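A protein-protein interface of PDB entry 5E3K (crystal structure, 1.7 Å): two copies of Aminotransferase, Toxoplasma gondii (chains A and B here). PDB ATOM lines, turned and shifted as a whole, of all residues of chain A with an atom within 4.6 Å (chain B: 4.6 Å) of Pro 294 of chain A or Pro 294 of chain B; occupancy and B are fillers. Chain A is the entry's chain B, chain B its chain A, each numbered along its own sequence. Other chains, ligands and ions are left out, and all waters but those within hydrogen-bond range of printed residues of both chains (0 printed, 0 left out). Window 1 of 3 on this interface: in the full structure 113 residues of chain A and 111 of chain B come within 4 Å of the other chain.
Of the printed residues of chain B, Asn 134 of chain A touches Pro 294. Asn 320 of chain A touches none of the printed residues of chain B. Of the printed residues of chain A, Asn 134 of chain B touches Thr 135 (3.5 Å) and Pro 294 (3.7 Å). Of the printed residues of chain A, Pro 294 of chain B touches Asn 134, Pro 294 and Phe 317. Ile 295 of chain B touches none of the printed residues of chain A. The nearest printed residue of chain B that does not touch Pro 294 of chain A is Val 293 of chain B (5.2 Å). The nearest printed residue of chain B that does not touch Asn 134 of chain A is Asn 134 of chain B (5.3 Å).
O of Asn 134 of chain B lies within hydrogen-bond range of N of Ile 295 of chain B (3.0 Å). The side-chain amide oxygen of Asn 134 of chain B lies close to the backbone carbonyl oxygen of Phe 317 of chain B (3.3 Å). The backbone NH of Ile 295 of chain A lies within hydrogen-bond range of the backbone carbonyl oxygen of Asn 134 of chain A (3.1 Å). N of Asn 134 of chain A sits at hydrogen-bond distance from OG of Ser 296 of chain A (3.4 Å). The side-chain amide oxygen (OD1) of Asn 134 of chain A sits close to the backbone carbonyl oxygen (O) of Phe 317 of chain A (3.3 Å). The backbone carbonyl oxygen (O) of Thr 135 of chain A is in hydrogen-bond range of the side-chain hydroxyl (OG) of Ser 296 of chain A.
Asn 134 of chain A touches Pro 294 of chain B, and with the chains exchanged Pro 294 of chain A touches Asn 134 of chain B. Val 293 of chain A touches its own counterpart, Val 293 of chain B. Pro 294 of chain A touches its own counterpart, Pro 294 of chain B. Pro 294 of chain A touches Phe 317 of chain B, and with the chains exchanged Phe 317 of chain A touches Pro 294 of chain B. Of the 9 pairs that touch across the chains among the printed residues, 8 have their exchanged pair printed and touching as well.
Of the 6 printed residues of chain B, 4 touch a printed residue of chain A. Printed residues of chain A that touch a printed residue of chain B: Asn 134, Thr 135, Val 293, Pro 294 and Phe 317. Hydrophobic or aromatic side chains of chain A within 4 Å of the printed part of chain B: Val 293, Pro 294 and Phe 317. Among the printed residues, 9 pairs touch across the chains. Among the printed residues, no Asp or Glu carboxylate lies within 4 Å of a Lys or Arg side-chain nitrogen of the other chain.
Among the printed residues, merely in contact across the chains: Val 293 of chain A with Val 293 of chain B, Thr 135 of chain A with Asn 134 of chain B, Pro 294 of chain A with Asn 134 of chain B, Pro 294 of chain A with Phe 317 of chain B, Asn 134 of chain A with Pro 294 of chain B, Phe 317 of chain A with Pro 294 of chain B, Phe 317 of chain A with Val 293 of chain B, Val 293 of chain A with Phe 317 of chain B and Pro 294 of chain A with Pro 294 of chain B.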
ATOM      1  N   ASN A 134     -25.829  -1.990  26.576  1.00  0.00           N
ATOM      2  CA  ASN A 134     -25.175  -3.287  26.617  1.00  0.00           C
ATOM      3  C   ASN A 134     -23.927  -3.327  27.462  1.00  0.00           C
ATOM      4  O   ASN A 134     -23.750  -4.245  28.281  1.00  0.00           O
ATOM      5  CB  ASN A 134     -24.894  -3.808  25.173  1.00  0.00           C
ATOM      6  CG  ASN A 134     -26.088  -3.715  24.316  1.00  0.00           C
ATOM      7  OD1 ASN A 134     -26.962  -4.604  24.380  1.00  0.00           O
ATOM      8  ND2 ASN A 134     -26.264  -2.552  23.635  1.00  0.00           N
ATOM      9  N   THR A 135     -23.075  -2.310  27.359  1.00  0.00           N
ATOM     10  CA  THR A 135     -21.806  -2.373  28.061  1.00  0.00           C
ATOM     11  C   THR A 135     -21.698  -1.156  29.000  1.00  0.00           C
ATOM     12  O   THR A 135     -22.482  -0.200  28.924  1.00  0.00           O
ATOM     13  CB  THR A 135     -20.634  -2.329  27.069  1.00  0.00           C
ATOM     14  OG1 THR A 135     -20.609  -1.095  26.368  1.00  0.00           O
ATOM     15  CG2 THR A 135     -20.709  -3.462  26.062  1.00  0.00           C
ATOM     16  N   VAL A 293     -24.382 -12.178  30.251  1.00  0.00           N
ATOM     17  CA  VAL A 293     -24.497 -11.502  28.963  1.00  0.00           C
ATOM     18  C   VAL A 293     -24.331  -9.986  29.242  1.00  0.00           C
ATOM     19  O   VAL A 293     -24.629  -9.513  30.340  1.00  0.00           O
ATOM     20  CB  VAL A 293     -25.845 -11.723  28.273  1.00  0.00           C
ATOM     21  CG1 VAL A 293     -26.074 -13.190  27.824  1.00  0.00           C
ATOM     22  CG2 VAL A 293     -26.992 -11.227  29.133  1.00  0.00           C
ATOM     23  N   PRO A 294     -23.918  -9.214  28.229  1.00  0.00           N
ATOM     24  CA  PRO A 294     -23.660  -7.803  28.548  1.00  0.00           C
ATOM     25  C   PRO A 294     -24.974  -7.007  28.625  1.00  0.00           C
ATOM     26  O   PRO A 294     -25.691  -7.003  27.651  1.00  0.00           O
ATOM     27  CB  PRO A 294     -22.817  -7.309  27.361  1.00  0.00           C
ATOM     28  CG  PRO A 294     -22.547  -8.485  26.510  1.00  0.00           C
ATOM     29  CD  PRO A 294     -23.354  -9.639  26.924  1.00  0.00           C
ATOM     30  N   ILE A 295     -25.289  -6.447  29.772  1.00  0.00           N
ATOM     31  CA  ILE A 295     -26.431  -5.514  29.904  1.00  0.00           C
ATOM     32  C   ILE A 295     -25.982  -4.449  30.893  1.00  0.00           C
ATOM     33  O   ILE A 295     -25.454  -4.769  31.966  1.00  0.00           O
ATOM     34  CB  ILE A 295     -27.781  -6.217  30.297  1.00  0.00           C
ATOM     35  CG1 ILE A 295     -28.842  -5.209  30.753  1.00  0.00           C
ATOM     36  CG2 ILE A 295     -27.591  -7.307  31.321  1.00  0.00           C
ATOM     37  CD1 ILE A 295     -30.276  -5.701  30.727  1.00  0.00           C
ATOM     38  N   SER A 296     -26.275  -3.191  30.583  1.00  0.00           N
ATOM     39  CA  SER A 296     -25.964  -2.058  31.463  1.00  0.00           C
ATOM     40  C   SER A 296     -27.183  -1.172  31.558  1.00  0.00           C
ATOM     41  O   SER A 296     -28.128  -1.320  30.760  1.00  0.00           O
ATOM     42  CB  SER A 296     -24.769  -1.264  30.915  1.00  0.00           C
ATOM     43  OG  SER A 296     -25.085  -0.736  29.633  1.00  0.00           O
ATOM     44  N   PHE A 317     -29.094  -4.110  20.461  1.00  0.00           N
ATOM     45  CA  PHE A 317     -29.362  -5.069  21.530  1.00  0.00           C
ATOM     46  C   PHE A 317     -29.821  -4.508  22.885  1.00  0.00           C
ATOM     47  O   PHE A 317     -30.163  -5.280  23.798  1.00  0.00           O
ATOM     48  CB  PHE A 317     -28.135  -5.990  21.752  1.00  0.00           C
ATOM     49  CG  PHE A 317     -27.943  -7.006  20.666  1.00  0.00           C
ATOM     50  CD1 PHE A 317     -27.236  -6.708  19.540  1.00  0.00           C
ATOM     51  CD2 PHE A 317     -28.503  -8.266  20.790  1.00  0.00           C
ATOM     52  CE1 PHE A 317     -27.052  -7.646  18.538  1.00  0.00           C
ATOM     53  CE2 PHE A 317     -28.360  -9.197  19.798  1.00  0.00           C
ATOM     54  CZ  PHE A 317     -27.625  -8.901  18.662  1.00  0.00           C
ATOM     55  N   ASN A 320     -32.794  -5.957  25.118  1.00  0.00           N
ATOM     56  CA  ASN A 320     -33.293  -7.191  24.552  1.00  0.00           C
ATOM     57  C   ASN A 320     -33.914  -8.045  25.653  1.00  0.00           C
ATOM     58  O   ASN A 320     -33.394  -8.101  26.769  1.00  0.00           O
ATOM     59  CB  ASN A 320     -32.222  -7.915  23.743  1.00  0.00           C
ATOM     60  CG  ASN A 320     -31.168  -8.595  24.600  1.00  0.00           C
ATOM     61  OD1 ASN A 320     -31.381  -9.700  25.070  1.00  0.00           O
ATOM     62  ND2 ASN A 320     -30.014  -7.978  24.739  1.00  0.00           N
ATOM     63  N   ASN B 134     -18.668  -5.922  21.721  1.00  0.00           N
ATOM     64  CA  ASN B 134     -20.002  -6.355  22.096  1.00  0.00           C
ATOM     65  C   ASN B 134     -21.056  -5.818  21.155  1.00  0.00           C
ATOM     66  O   ASN B 134     -21.891  -6.604  20.688  1.00  0.00           O
ATOM     67  CB  ASN B 134     -20.348  -6.003  23.544  1.00  0.00           C
ATOM     68  CG  ASN B 134     -19.322  -6.538  24.497  1.00  0.00           C
ATOM     69  OD1 ASN B 134     -19.332  -7.717  24.807  1.00  0.00           O
ATOM     70  ND2 ASN B 134     -18.355  -5.693  24.852  1.00  0.00           N
ATOM     71  N   VAL B 293     -27.191 -12.820  21.691  1.00  0.00           N
ATOM     72  CA  VAL B 293     -26.435 -12.010  22.641  1.00  0.00           C
ATOM     73  C   VAL B 293     -25.599 -11.013  21.828  1.00  0.00           C
ATOM     74  O   VAL B 293     -25.175 -11.288  20.725  1.00  0.00           O
ATOM     75  CB  VAL B 293     -25.483 -12.858  23.510  1.00  0.00           C
ATOM     76  CG1 VAL B 293     -26.165 -13.834  24.490  1.00  0.00           C
ATOM     77  CG2 VAL B 293     -24.566 -13.716  22.686  1.00  0.00           C
ATOM     78  N   PRO B 294     -25.277  -9.854  22.385  1.00  0.00           N
ATOM     79  CA  PRO B 294     -24.474  -8.911  21.606  1.00  0.00           C
ATOM     80  C   PRO B 294     -23.000  -9.318  21.477  1.00  0.00           C
ATOM     81  O   PRO B 294     -22.321  -9.428  22.482  1.00  0.00           O
ATOM     82  CB  PRO B 294     -24.548  -7.634  22.401  1.00  0.00           C
ATOM     83  CG  PRO B 294     -25.234  -7.953  23.660  1.00  0.00           C
ATOM     84  CD  PRO B 294     -25.788  -9.297  23.657  1.00  0.00           C
ATOM     85  N   ILE B 295     -22.543  -9.538  20.255  1.00  0.00           N
ATOM     86  CA  ILE B 295     -21.103  -9.750  19.967  1.00  0.00           C
ATOM     87  C   ILE B 295     -20.819  -9.151  18.642  1.00  0.00           C
ATOM     88  O   ILE B 295     -21.592  -9.327  17.707  1.00  0.00           O
ATOM     89  CB  ILE B 295     -20.653 -11.239  20.078  1.00  0.00           C
ATOM     90  CG1 ILE B 295     -19.274 -11.478  19.483  1.00  0.00           C
ATOM     91  CG2 ILE B 295     -21.714 -12.198  19.586  1.00  0.00           C
ATOM     92  CD1 ILE B 295     -18.602 -12.756  19.996  1.00  0.00           C
ATOM     93  N   SER B 296     -19.704  -8.435  18.541  1.00  0.00           N
ATOM     94  CA  SER B 296     -19.322  -7.748  17.309  1.00  0.00           C
ATOM     95  C   SER B 296     -17.865  -8.093  17.066  1.00  0.00           C
ATOM     96  O   SER B 296     -17.172  -8.640  17.955  1.00  0.00           O
ATOM     97  CB  SER B 296     -19.582  -6.242  17.443  1.00  0.00           C
ATOM     98  OG  SER B 296     -18.777  -5.643  18.407  1.00  0.00           O
ATOM     99  N   PHE B 317     -16.825  -7.480  28.597  1.00  0.00           N
ATOM    100  CA  PHE B 317     -17.508  -8.639  27.997  1.00  0.00           C
ATOM    101  C   PHE B 317     -16.995  -9.036  26.612  1.00  0.00           C
ATOM    102  O   PHE B 317     -17.394 -10.094  26.098  1.00  0.00           O
ATOM    103  CB  PHE B 317     -19.038  -8.411  27.992  1.00  0.00           C
ATOM    104  CG  PHE B 317     -19.677  -8.573  29.323  1.00  0.00           C
ATOM    105  CD1 PHE B 317     -20.175  -9.819  29.706  1.00  0.00           C
ATOM    106  CD2 PHE B 317     -19.925  -7.482  30.155  1.00  0.00           C
ATOM    107  CE1 PHE B 317     -20.811  -9.994  30.948  1.00  0.00           C
ATOM    108  CE2 PHE B 317     -20.540  -7.648  31.385  1.00  0.00           C
ATOM    109  CZ  PHE B 317     -21.045  -8.903  31.779  1.00  0.00           C
